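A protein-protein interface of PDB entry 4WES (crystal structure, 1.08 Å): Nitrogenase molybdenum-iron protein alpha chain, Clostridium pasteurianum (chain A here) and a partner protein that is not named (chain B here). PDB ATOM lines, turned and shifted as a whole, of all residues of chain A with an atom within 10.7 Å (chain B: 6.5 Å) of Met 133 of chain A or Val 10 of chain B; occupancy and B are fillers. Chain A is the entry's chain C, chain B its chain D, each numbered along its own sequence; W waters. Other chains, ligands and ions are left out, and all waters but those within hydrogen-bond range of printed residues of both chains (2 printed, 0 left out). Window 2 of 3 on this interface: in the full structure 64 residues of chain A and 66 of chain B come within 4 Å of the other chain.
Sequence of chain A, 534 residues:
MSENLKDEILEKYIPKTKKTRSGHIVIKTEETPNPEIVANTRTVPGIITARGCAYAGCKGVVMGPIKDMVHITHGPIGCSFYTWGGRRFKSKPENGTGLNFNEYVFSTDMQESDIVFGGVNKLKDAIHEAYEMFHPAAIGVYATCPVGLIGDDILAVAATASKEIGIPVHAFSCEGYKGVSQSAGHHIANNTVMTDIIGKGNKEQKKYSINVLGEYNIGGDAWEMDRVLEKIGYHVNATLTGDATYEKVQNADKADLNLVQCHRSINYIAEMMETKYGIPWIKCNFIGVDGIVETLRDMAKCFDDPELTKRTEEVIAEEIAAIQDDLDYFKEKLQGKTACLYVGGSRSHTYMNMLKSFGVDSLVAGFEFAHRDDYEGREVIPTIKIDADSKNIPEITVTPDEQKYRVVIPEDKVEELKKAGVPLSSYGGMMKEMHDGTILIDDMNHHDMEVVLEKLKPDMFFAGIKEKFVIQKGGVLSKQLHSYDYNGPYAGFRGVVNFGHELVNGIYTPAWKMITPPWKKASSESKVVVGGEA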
ATOM      1  N   VAL A  70       8.555  24.570   4.787  1.00  0.00           N
ATOM      2  CA  VAL A  70       7.739  24.631   3.583  1.00  0.00           C
ATOM      3  C   VAL A  70       6.269  24.679   3.985  1.00  0.00           C
ATOM      4  O   VAL A  70       5.771  23.764   4.661  1.00  0.00           O
ATOM      5  CB  VAL A  70       7.994  23.447   2.634  1.00  0.00           C
ATOM      6  CG1 VAL A  70       6.902  23.327   1.556  1.00  0.00           C
ATOM      7  CG2 VAL A  70       9.352  23.593   1.993  1.00  0.00           C
ATOM      8  N   ILE A  72       2.560  24.560   2.956  1.00  0.00           N
ATOM      9  CA  ILE A  72       1.680  24.102   1.911  1.00  0.00           C
ATOM     10  C   ILE A  72       0.242  24.501   2.203  1.00  0.00           C
ATOM     11  O   ILE A  72      -0.351  24.031   3.180  1.00  0.00           O
ATOM     12  CB  ILE A  72       1.761  22.570   1.724  1.00  0.00           C
ATOM     13  CG1 ILE A  72       3.209  22.135   1.456  1.00  0.00           C
ATOM     14  CG2 ILE A  72       0.858  22.138   0.573  1.00  0.00           C
ATOM     15  CD1 ILE A  72       3.398  20.625   1.362  1.00  0.00           C
ATOM     16  N   LEU A  99      18.231  27.381   4.463  1.00  0.00           N
ATOM     17  CA  LEU A  99      17.116  27.419   3.529  1.00  0.00           C
ATOM     18  C   LEU A  99      16.266  28.653   3.695  1.00  0.00           C
ATOM     19  O   LEU A  99      16.124  29.173   4.810  1.00  0.00           O
ATOM     20  CB  LEU A  99      16.237  26.184   3.740  1.00  0.00           C
ATOM     21  CG  LEU A  99      16.924  24.847   3.469  1.00  0.00           C
ATOM     22  CD1 LEU A  99      16.029  23.710   3.921  1.00  0.00           C
ATOM     23  CD2 LEU A  99      17.237  24.671   2.005  1.00  0.00           C
ATOM     24  N   PHE A 101      12.503  29.924   1.905  1.00  0.00           N
ATOM     25  CA  PHE A 101      11.426  29.726   0.932  1.00  0.00           C
ATOM     26  C   PHE A 101      10.548  30.959   0.710  1.00  0.00           C
ATOM     27  O   PHE A 101       9.455  30.853   0.120  1.00  0.00           O
ATOM     28  CB  PHE A 101      10.573  28.497   1.278  1.00  0.00           C
ATOM     29  CG  PHE A 101      11.395  27.240   1.409  1.00  0.00           C
ATOM     30  CD1 PHE A 101      11.973  26.658   0.293  1.00  0.00           C
ATOM     31  CD2 PHE A 101      11.651  26.669   2.640  1.00  0.00           C
ATOM     32  CE1 PHE A 101      12.759  25.547   0.399  1.00  0.00           C
ATOM     33  CE2 PHE A 101      12.449  25.527   2.766  1.00  0.00           C
ATOM     34  CZ  PHE A 101      13.008  24.968   1.635  1.00  0.00           C
ATOM     35  N   TYR A 104       8.725  31.653  -2.687  1.00  0.00           N
ATOM     36  CA  TYR A 104       7.861  30.602  -3.226  1.00  0.00           C
ATOM     37  C   TYR A 104       6.522  30.580  -2.517  1.00  0.00           C
ATOM     38  O   TYR A 104       6.419  30.932  -1.362  1.00  0.00           O
ATOM     39  CB  TYR A 104       8.492  29.223  -3.003  1.00  0.00           C
ATOM     40  CG  TYR A 104       9.823  29.039  -3.638  1.00  0.00           C
ATOM     41  CD1 TYR A 104      10.987  29.418  -2.962  1.00  0.00           C
ATOM     42  CD2 TYR A 104       9.962  28.470  -4.871  1.00  0.00           C
ATOM     43  CE1 TYR A 104      12.236  29.251  -3.553  1.00  0.00           C
ATOM     44  CE2 TYR A 104      11.208  28.310  -5.469  1.00  0.00           C
ATOM     45  CZ  TYR A 104      12.353  28.675  -4.783  1.00  0.00           C
ATOM     46  OH  TYR A 104      13.592  28.509  -5.329  1.00  0.00           O
ATOM     47  N   VAL A 105       5.502  30.088  -3.227  1.00  0.00           N
ATOM     48  CA  VAL A 105       4.285  29.612  -2.560  1.00  0.00           C
ATOM     49  C   VAL A 105       3.975  28.214  -3.043  1.00  0.00           C
ATOM     50  O   VAL A 105       4.163  27.878  -4.223  1.00  0.00           O
ATOM     51  CB  VAL A 105       3.057  30.535  -2.747  1.00  0.00           C
ATOM     52  CG1 VAL A 105       3.231  31.813  -1.959  1.00  0.00           C
ATOM     53  CG2 VAL A 105       2.738  30.824  -4.207  1.00  0.00           C
ATOM     54  N   PHE A 106       3.481  27.415  -2.100  1.00  0.00           N
ATOM     55  CA  PHE A 106       3.235  25.986  -2.304  1.00  0.00           C
ATOM     56  C   PHE A 106       1.777  25.665  -2.017  1.00  0.00           C
ATOM     57  O   PHE A 106       1.210  26.143  -1.022  1.00  0.00           O
ATOM     58  CB  PHE A 106       4.093  25.193  -1.317  1.00  0.00           C
ATOM     59  CG  PHE A 106       5.577  25.441  -1.438  1.00  0.00           C
ATOM     60  CD1 PHE A 106       6.277  24.887  -2.461  1.00  0.00           C
ATOM     61  CD2 PHE A 106       6.231  26.247  -0.523  1.00  0.00           C
ATOM     62  CE1 PHE A 106       7.640  25.129  -2.605  1.00  0.00           C
ATOM     63  CE2 PHE A 106       7.584  26.459  -0.649  1.00  0.00           C
ATOM     64  CZ  PHE A 106       8.276  25.929  -1.698  1.00  0.00           C
ATOM     65  N   ASP A 125       0.542  13.369  -1.336  1.00  0.00           N
ATOM     66  CA  ASP A 125       1.512  13.359  -2.425  1.00  0.00           C
ATOM     67  C   ASP A 125       2.299  14.662  -2.479  1.00  0.00           C
ATOM     68  O   ASP A 125       3.500  14.653  -2.761  1.00  0.00           O
ATOM     69  CB  ASP A 125       0.804  13.109  -3.758  1.00  0.00           C
ATOM     70  CG  ASP A 125       0.252  11.700  -3.901  1.00  0.00           C
ATOM     71  OD1 ASP A 125       0.568  10.835  -3.060  1.00  0.00           O
ATOM     72  OD2 ASP A 125      -0.497  11.493  -4.886  1.00  0.00           O
ATOM     73  N   ALA A 126       1.624  15.786  -2.212  1.00  0.00           N
ATOM     74  CA  ALA A 126       2.301  17.080  -2.219  1.00  0.00           C
ATOM     75  C   ALA A 126       3.315  17.209  -1.101  1.00  0.00           C
ATOM     76  O   ALA A 126       4.390  17.786  -1.320  1.00  0.00           O
ATOM     77  CB  ALA A 126       1.299  18.210  -2.154  1.00  0.00           C
ATOM     78  N   ILE A 127       2.998  16.683   0.076  1.00  0.00           N
ATOM     79  CA  ILE A 127       3.942  16.720   1.199  1.00  0.00           C
ATOM     80  C   ILE A 127       5.189  15.924   0.812  1.00  0.00           C
ATOM     81  O   ILE A 127       6.311  16.386   1.043  1.00  0.00           O
ATOM     82  CB  ILE A 127       3.316  16.128   2.469  1.00  0.00           C
ATOM     83  CG1 ILE A 127       2.178  17.015   2.997  1.00  0.00           C
ATOM     84  CG2 ILE A 127       4.350  15.876   3.548  1.00  0.00           C
ATOM     85  CD1 ILE A 127       1.255  16.338   3.983  1.00  0.00           C
ATOM     86  N   HIS A 128       4.990  14.745   0.253  1.00  0.00           N
ATOM     87  CA  HIS A 128       6.155  13.946  -0.152  1.00  0.00           C
ATOM     88  C   HIS A 128       6.947  14.640  -1.260  1.00  0.00           C
ATOM     89  O   HIS A 128       8.184  14.616  -1.203  1.00  0.00           O
ATOM     90  CB  HIS A 128       5.716  12.563  -0.566  1.00  0.00           C
ATOM     91  CG  HIS A 128       5.433  11.651   0.593  1.00  0.00           C
ATOM     92  ND1 HIS A 128       6.363  10.797   1.108  1.00  0.00           N
ATOM     93  CD2 HIS A 128       4.330  11.497   1.358  1.00  0.00           C
ATOM     94  CE1 HIS A 128       5.834  10.132   2.118  1.00  0.00           C
ATOM     95  NE2 HIS A 128       4.605  10.562   2.305  1.00  0.00           N
ATOM     96  N   GLU A 129       6.288  15.242  -2.261  1.00  0.00           N
ATOM     97  CA  GLU A 129       7.025  15.932  -3.296  1.00  0.00           C
ATOM     98  C   GLU A 129       7.825  17.081  -2.704  1.00  0.00           C
ATOM     99  O   GLU A 129       8.992  17.282  -3.107  1.00  0.00           O
ATOM    100  CB  GLU A 129       6.098  16.442  -4.421  1.00  0.00           C
ATOM    101  CG  GLU A 129       5.610  15.323  -5.314  1.00  0.00           C
ATOM    102  CD  GLU A 129       4.703  15.715  -6.437  1.00  0.00           C
ATOM    103  OE1 GLU A 129       4.181  16.851  -6.466  1.00  0.00           O
ATOM    104  OE2 GLU A 129       4.508  14.847  -7.333  1.00  0.00           O
ATOM    105  N   ALA A 130       7.244  17.825  -1.768  1.00  0.00           N
ATOM    106  CA  ALA A 130       7.958  18.931  -1.141  1.00  0.00           C
ATOM    107  C   ALA A 130       9.172  18.425  -0.346  1.00  0.00           C
ATOM    108  O   ALA A 130      10.252  19.024  -0.390  1.00  0.00           O
ATOM    109  CB  ALA A 130       7.030  19.693  -0.229  1.00  0.00           C
ATOM    110  N   TYR A 131       8.991  17.341   0.410  1.00  0.00           N
ATOM    111  CA  TYR A 131      10.103  16.775   1.182  1.00  0.00           C
ATOM    112  C   TYR A 131      11.238  16.366   0.254  1.00  0.00           C
ATOM    113  O   TYR A 131      12.395  16.713   0.473  1.00  0.00           O
ATOM    114  CB  TYR A 131       9.607  15.586   2.003  1.00  0.00           C
ATOM    115  CG  TYR A 131      10.777  14.880   2.647  1.00  0.00           C
ATOM    116  CD1 TYR A 131      11.451  15.456   3.714  1.00  0.00           C
ATOM    117  CD2 TYR A 131      11.263  13.681   2.153  1.00  0.00           C
ATOM    118  CE1 TYR A 131      12.565  14.848   4.280  1.00  0.00           C
ATOM    119  CE2 TYR A 131      12.361  13.077   2.704  1.00  0.00           C
ATOM    120  CZ  TYR A 131      12.998  13.667   3.756  1.00  0.00           C
ATOM    121  OH  TYR A 131      14.099  13.038   4.313  1.00  0.00           O
ATOM    122  N   GLU A 132      10.922  15.586  -0.772  1.00  0.00           N
ATOM    123  CA  GLU A 132      11.952  15.067  -1.661  1.00  0.00           C
ATOM    124  C   GLU A 132      12.679  16.168  -2.399  1.00  0.00           C
ATOM    125  O   GLU A 132      13.867  16.051  -2.707  1.00  0.00           O
ATOM    126  CB  GLU A 132      11.348  14.073  -2.642  1.00  0.00           C
ATOM    127  CG  GLU A 132      10.780  12.813  -1.997  1.00  0.00           C
ATOM    128  CD  GLU A 132      11.772  11.953  -1.268  1.00  0.00           C
ATOM    129  OE1 GLU A 132      13.006  12.043  -1.520  1.00  0.00           O
ATOM    130  OE2 GLU A 132      11.305  11.133  -0.430  1.00  0.00           O
ATOM    131  N   MET A 133      11.955  17.232  -2.759  1.00  0.00           N
ATOM    132  CA  MET A 133      12.537  18.308  -3.544  1.00  0.00           C
ATOM    133  C   MET A 133      13.334  19.305  -2.695  1.00  0.00           C
ATOM    134  O   MET A 133      14.321  19.869  -3.197  1.00  0.00           O
ATOM    135  CB  MET A 133      11.435  19.025  -4.327  1.00  0.00           C
ATOM    136  CG  MET A 133      11.951  19.978  -5.351  1.00  0.00           C
ATOM    137  SD  MET A 133      10.690  20.456  -6.566  1.00  0.00           S
ATOM    138  CE  MET A 133      10.040  18.898  -7.018  1.00  0.00           C
ATOM    139  N   PHE A 134      12.885  19.572  -1.480  1.00  0.00           N
ATOM    140  CA  PHE A 134      13.407  20.689  -0.695  1.00  0.00           C
ATOM    141  C   PHE A 134      14.082  20.318   0.608  1.00  0.00           C
ATOM    142  O   PHE A 134      14.817  21.156   1.135  1.00  0.00           O
ATOM    143  CB  PHE A 134      12.277  21.715  -0.437  1.00  0.00           C
ATOM    144  CG  PHE A 134      11.673  22.272  -1.692  1.00  0.00           C
ATOM    145  CD1 PHE A 134      12.432  23.036  -2.541  1.00  0.00           C
ATOM    146  CD2 PHE A 134      10.387  21.960  -2.072  1.00  0.00           C
ATOM    147  CE1 PHE A 134      11.914  23.548  -3.698  1.00  0.00           C
ATOM    148  CE2 PHE A 134       9.844  22.470  -3.259  1.00  0.00           C
ATOM    149  CZ  PHE A 134      10.617  23.249  -4.066  1.00  0.00           C
ATOM    150  N   HIS A 135      13.790  19.139   1.149  1.00  0.00           N
ATOM    151  CA  HIS A 135      14.344  18.715   2.456  1.00  0.00           C
ATOM    152  C   HIS A 135      14.359  19.853   3.469  1.00  0.00           C
ATOM    153  O   HIS A 135      15.404  20.230   4.000  1.00  0.00           O
ATOM    154  CB  HIS A 135      15.725  18.085   2.301  1.00  0.00           C
ATOM    155  CG  HIS A 135      15.680  16.815   1.517  1.00  0.00           C
ATOM    156  ND1 HIS A 135      15.848  16.777   0.160  1.00  0.00           N
ATOM    157  CD2 HIS A 135      15.372  15.552   1.885  1.00  0.00           C
ATOM    158  CE1 HIS A 135      15.712  15.542  -0.273  1.00  0.00           C
ATOM    159  NE2 HIS A 135      15.408  14.781   0.755  1.00  0.00           N
ATOM    160  N   PRO A 136      13.178  20.385   3.800  1.00  0.00           N
ATOM    161  CA  PRO A 136      13.092  21.515   4.706  1.00  0.00           C
ATOM    162  C   PRO A 136      13.207  21.087   6.169  1.00  0.00           C
ATOM    163  O   PRO A 136      13.243  19.895   6.482  1.00  0.00           O
ATOM    164  CB  PRO A 136      11.693  22.079   4.423  1.00  0.00           C
ATOM    165  CG  PRO A 136      10.898  20.831   4.153  1.00  0.00           C
ATOM    166  CD  PRO A 136      11.838  19.939   3.365  1.00  0.00           C
ATOM    167  N   ALA A 137      13.246  22.067   7.073  1.00  0.00           N
ATOM    168  CA  ALA A 137      13.278  21.758   8.490  1.00  0.00           C
ATOM    169  C   ALA A 137      11.973  21.118   8.980  1.00  0.00           C
ATOM    170  O   ALA A 137      11.960  20.308   9.906  1.00  0.00           O
ATOM    171  CB  ALA A 137      13.535  23.033   9.288  1.00  0.00           C
ATOM    172  N   ILE A 139       7.412  20.883   7.575  1.00  0.00           N
ATOM    173  CA  ILE A 139       6.375  21.243   6.599  1.00  0.00           C
ATOM    174  C   ILE A 139       5.130  21.649   7.377  1.00  0.00           C
ATOM    175  O   ILE A 139       4.769  21.010   8.359  1.00  0.00           O
ATOM    176  CB  ILE A 139       6.097  20.044   5.647  1.00  0.00           C
ATOM    177  CG1 ILE A 139       7.313  19.804   4.758  1.00  0.00           C
ATOM    178  CG2 ILE A 139       4.838  20.278   4.799  1.00  0.00           C
ATOM    179  CD1 ILE A 139       7.279  18.533   3.955  1.00  0.00           C
ATOM    180  N   ILE A 165       8.379  10.513   6.374  1.00  0.00           N
ATOM    181  CA  ILE A 165       9.500  11.304   5.866  1.00  0.00           C
ATOM    182  C   ILE A 165      10.536  11.643   6.926  1.00  0.00           C
ATOM    183  O   ILE A 165      11.641  12.016   6.574  1.00  0.00           O
ATOM    184  CB  ILE A 165       9.044  12.584   5.129  1.00  0.00           C
ATOM    185  CG1 ILE A 165       8.376  13.583   6.085  1.00  0.00           C
ATOM    186  CG2 ILE A 165       8.128  12.229   3.956  1.00  0.00           C
ATOM    187  CD1 ILE A 165       7.892  14.846   5.410  1.00  0.00           C
ATOM    188  N   ILE A 167      10.572  14.131   9.292  1.00  0.00           N
ATOM    189  CA  ILE A 167      10.686  15.507   9.750  1.00  0.00           C
ATOM    190  C   ILE A 167       9.304  15.920  10.249  1.00  0.00           C
ATOM    191  O   ILE A 167       8.300  15.282   9.931  1.00  0.00           O
ATOM    192  CB  ILE A 167      11.190  16.498   8.667  1.00  0.00           C
ATOM    193  CG1 ILE A 167      10.216  16.609   7.496  1.00  0.00           C
ATOM    194  CG2 ILE A 167      12.611  16.156   8.211  1.00  0.00           C
ATOM    195  CD1 ILE A 167      10.467  17.796   6.597  1.00  0.00           C
ATOM    196  N   ALA B   4      16.431  27.422  -4.107  1.00  0.00           N
ATOM    197  CA  ALA B   4      15.909  26.078  -3.883  1.00  0.00           C
ATOM    198  C   ALA B   4      15.414  25.383  -5.149  1.00  0.00           C
ATOM    199  O   ALA B   4      14.990  24.232  -5.082  1.00  0.00           O
ATOM    200  CB  ALA B   4      14.789  26.131  -2.865  1.00  0.00           C
ATOM    201  N   PRO B   6      15.865  23.345  -8.294  1.00  0.00           N
ATOM    202  CA  PRO B   6      16.946  22.545  -8.890  1.00  0.00           C
ATOM    203  C   PRO B   6      16.964  22.599 -10.420  1.00  0.00           C
ATOM    204  O   PRO B   6      15.920  22.773 -11.055  1.00  0.00           O
ATOM    205  CB  PRO B   6      16.620  21.119  -8.407  1.00  0.00           C
ATOM    206  CG  PRO B   6      15.497  21.205  -7.443  1.00  0.00           C
ATOM    207  CD  PRO B   6      14.806  22.478  -7.737  1.00  0.00           C
ATOM    208  N   GLU B   8      17.976  19.842 -12.060  1.00  0.00           N
ATOM    209  CA  GLU B   8      17.518  18.515 -12.424  1.00  0.00           C
ATOM    210  C   GLU B   8      16.040  18.394 -12.085  1.00  0.00           C
ATOM    211  O   GLU B   8      15.643  18.597 -10.973  1.00  0.00           O
ATOM    212  CB  GLU B   8      18.332  17.471 -11.645  1.00  0.00           C
ATOM    213  CG  GLU B   8      19.850  17.644 -11.693  1.00  0.00           C
ATOM    214  CD  GLU B   8      20.483  18.902 -10.989  1.00  0.00           C
ATOM    215  OE1 GLU B   8      19.928  19.560  -9.978  1.00  0.00           O
ATOM    216  OE2 GLU B   8      21.621  19.192 -11.510  1.00  0.00           O
ATOM    217  N   ILE B   9      15.237  18.060 -13.093  1.00  0.00           N
ATOM    218  CA  ILE B   9      13.792  18.089 -12.964  1.00  0.00           C
ATOM    219  C   ILE B   9      13.247  16.736 -12.515  1.00  0.00           C
ATOM    220  O   ILE B   9      13.495  15.714 -13.152  1.00  0.00           O
ATOM    221  CB  ILE B   9      13.119  18.516 -14.294  1.00  0.00           C
ATOM    222  CG1 ILE B   9      13.613  19.902 -14.709  1.00  0.00           C
ATOM    223  CG2 ILE B   9      11.617  18.449 -14.180  1.00  0.00           C
ATOM    224  CD1 ILE B   9      13.191  20.341 -16.085  1.00  0.00           C
ATOM    225  N   VAL B  10      12.454  16.764 -11.448  1.00  0.00           N
ATOM    226  CA  VAL B  10      11.621  15.657 -11.017  1.00  0.00           C
ATOM    227  C   VAL B  10      10.201  16.192 -11.204  1.00  0.00           C
ATOM    228  O   VAL B  10       9.797  17.173 -10.572  1.00  0.00           O
ATOM    229  CB  VAL B  10      11.894  15.271  -9.555  1.00  0.00           C
ATOM    230  CG1 VAL B  10      10.975  14.175  -9.075  1.00  0.00           C
ATOM    231  CG2 VAL B  10      13.334  14.830  -9.385  1.00  0.00           C
ATOM    232  N   GLU B  11       9.452  15.509 -12.023  1.00  0.00           N
ATOM    233  CA  GLU B  11       8.115  15.995 -12.410  1.00  0.00           C
ATOM    234  C   GLU B  11       7.134  15.951 -11.229  1.00  0.00           C
ATOM    235  O   GLU B  11       7.053  14.966 -10.519  1.00  0.00           O
ATOM    236  CB  GLU B  11       7.535  15.251 -13.620  1.00  0.00           C
ATOM    237  CG  GLU B  11       6.086  15.620 -13.985  1.00  0.00           C
ATOM    238  CD  GLU B  11       5.480  14.746 -15.083  1.00  0.00           C
ATOM    239  OE1 GLU B  11       6.182  14.441 -16.074  1.00  0.00           O
ATOM    240  OE2 GLU B  11       4.291  14.380 -14.953  1.00  0.00           O
ATOM    241  N   ARG B  12       6.461  17.081 -10.990  1.00  0.00           N
ATOM    242  CA  ARG B  12       5.525  17.163  -9.909  1.00  0.00           C
ATOM    243  C   ARG B  12       4.148  16.828 -10.420  1.00  0.00           C
ATOM    244  O   ARG B  12       3.744  17.320 -11.461  1.00  0.00           O
ATOM    245  CB  ARG B  12       5.494  18.619  -9.287  1.00  0.00           C
ATOM    246  CG  ARG B  12       6.715  18.976  -8.550  1.00  0.00           C
ATOM    247  CD  ARG B  12       6.821  20.432  -8.359  1.00  0.00           C
ATOM    248  NE  ARG B  12       7.058  21.155  -9.607  1.00  0.00           N
ATOM    249  CZ  ARG B  12       6.335  22.160 -10.103  1.00  0.00           C
ATOM    250  NH1 ARG B  12       5.253  22.591  -9.488  1.00  0.00           N
ATOM    251  NH2 ARG B  12       6.716  22.747 -11.195  1.00  0.00           N
ATOM    252  N   LEU B  15       2.271  18.899  -6.073  1.00  0.00           N
ATOM    253  CA  LEU B  15       2.703  20.159  -5.485  1.00  0.00           C
ATOM    254  C   LEU B  15       2.786  21.268  -6.522  1.00  0.00           C
ATOM    255  O   LEU B  15       3.630  21.226  -7.425  1.00  0.00           O
ATOM    256  CB  LEU B  15       4.052  19.956  -4.835  1.00  0.00           C
ATOM    257  CG  LEU B  15       4.646  21.141  -4.061  1.00  0.00           C
ATOM    258  CD1 LEU B  15       3.871  21.428  -2.800  1.00  0.00           C
ATOM    259  CD2 LEU B  15       6.105  20.843  -3.744  1.00  0.00           C
ATOM    260  N   ILE B  17       3.648  25.102  -7.444  1.00  0.00           N
ATOM    261  CA  ILE B  17       4.625  26.052  -6.923  1.00  0.00           C
ATOM    262  C   ILE B  17       4.580  27.275  -7.835  1.00  0.00           C
ATOM    263  O   ILE B  17       4.745  27.152  -9.039  1.00  0.00           O
ATOM    264  CB  ILE B  17       6.059  25.489  -6.943  1.00  0.00           C
ATOM    265  CG1 ILE B  17       6.153  24.137  -6.235  1.00  0.00           C
ATOM    266  CG2 ILE B  17       7.009  26.480  -6.310  1.00  0.00           C
ATOM    267  CD1 ILE B  17       7.492  23.438  -6.368  1.00  0.00           C
ATOM    268  N   PHE B 375       7.739  27.760 -11.616  1.00  0.00           N
ATOM    269  CA  PHE B 375       8.817  26.829 -11.211  1.00  0.00           C
ATOM    270  C   PHE B 375       9.235  25.994 -12.410  1.00  0.00           C
ATOM    271  O   PHE B 375      10.434  25.823 -12.688  1.00  0.00           O
ATOM    272  CB  PHE B 375       8.330  25.998 -10.031  1.00  0.00           C
ATOM    273  CG  PHE B 375       9.418  25.240  -9.314  1.00  0.00           C
ATOM    274  CD1 PHE B 375      10.037  25.802  -8.214  1.00  0.00           C
ATOM    275  CD2 PHE B 375       9.729  23.946  -9.664  1.00  0.00           C
ATOM    276  CE1 PHE B 375      10.961  25.050  -7.485  1.00  0.00           C
ATOM    277  CE2 PHE B 375      10.662  23.204  -8.953  1.00  0.00           C
ATOM    278  CZ  PHE B 375      11.272  23.753  -7.850  1.00  0.00           C
ATOM    279  N   GLN B 379      13.013  25.990 -14.150  1.00  0.00           N
ATOM    280  CA  GLN B 379      13.790  24.770 -14.345  1.00  0.00           C
ATOM    281  C   GLN B 379      14.200  24.589 -15.799  1.00  0.00           C
ATOM    282  O   GLN B 379      15.334  24.200 -16.109  1.00  0.00           O
ATOM    283  CB  GLN B 379      13.046  23.548 -13.826  1.00  0.00           C
ATOM    284  CG  GLN B 379      12.826  23.563 -12.318  1.00  0.00           C
ATOM    285  CD  GLN B 379      12.431  22.203 -11.806  1.00  0.00           C
ATOM    286  OE1 GLN B 379      11.308  21.746 -12.053  1.00  0.00           O
ATOM    287  NE2 GLN B 379      13.294  21.580 -11.055  1.00  0.00           N
HETATM  288  O   HOH W   1      15.818  22.228  -3.399  1.00  0.00           O
HETATM  289  O   HOH W   2       6.998  13.574  -8.077  1.00  0.00           O
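OH of Tyr 104 of chain A is in hydrogen-bond range of N of Ala 4 of chain B, 3.3 Å away.
The backbone NH of Leu 15 of chain B is in hydrogen-bond range of the side-chain carboxylate of Glu 129 of chain A.
Of the 11 printed residues of chain B, 6 touch a printed residue of chain A.
Hydrophobic or aromatic side chains of chain B that line the printed part of chain A: Ala 4, Leu 15, Ile 17 and Phe 375.
Along chain A the printed residues that touch a printed residue of chain B span positions 101 to 134.
Among the printed residues, 16 pairs touch across the chains.
Water W1 lies within hydrogen-bond range of the backbone carbonyl oxygen (O) of Ala 4 of chain B and the backbone carbonyl oxygen (O) of Met 133 of chain A.
Water W2 bridges the backbone carbonyl oxygen (O) of Glu 11 of chain B (2.8 Å) and the side-chain carboxylate (OE2) of Glu 129 of chain A (2.9 Å).
Of the printed residues of chain B, Tyr 104 of chain A touches Ala 4 (3.3 Å), Ile 17 (3.8 Å) and Phe 375 (3.8 Å).
Printed residues of chain B within 4 Å of Val 105 of chain A: Ile 17 (3.3 Å).
Of the printed residues of chain B, Ala 130 of chain A touches Leu 15.
Met 133 of chain A touches three residues of chain B.
Glu 8 of chain B touches none of the printed residues of chain A.
No residue of chain A comes within 4 Å of Ile 9 of chain B.
Of chain A, only Met 133 (3.96 Å) comes within 4 Å of Val 10 of chain B.
The nearest residue of chain A that does not touch Val 10 of chain B is Glu 132 of chain A (6.4 Å).
The nearest printed residue of chain A that does not touch Leu 15 of chain B is Phe 106 of chain A (4.1 Å).
Among the printed residues, merely in contact across the chains: Phe 101 of chain A with Ala 4 of chain B, Tyr 104 of chain A with Ile 17 of chain B, Tyr 104 of chain A with Phe 375 of chain B, Val 105 of chain A with Ile 17 of chain B, Phe 106 of chain A with Ile 17 of chain B, Ala 126 of chain A with Leu 15 of chain B, Glu 129 of chain A with Arg 12 of chain B, Ala 130 of chain A with Leu 15 of chain B, Met 133 of chain A with Val 10 of chain B, Met 133 of chain A with Arg 12 of chain B, Met 133 of chain A with Phe 375 of chain B, Phe 134 of chain A with Ala 4 of chain B, Phe 134 of chain A with Ile 17 of chain B and Phe 134 of chain A with Phe 375 of chain B.
O of Leu 15 of chain B lies within hydrogen-bond range of NH1 of Arg 12 of chain B (3.0 Å).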
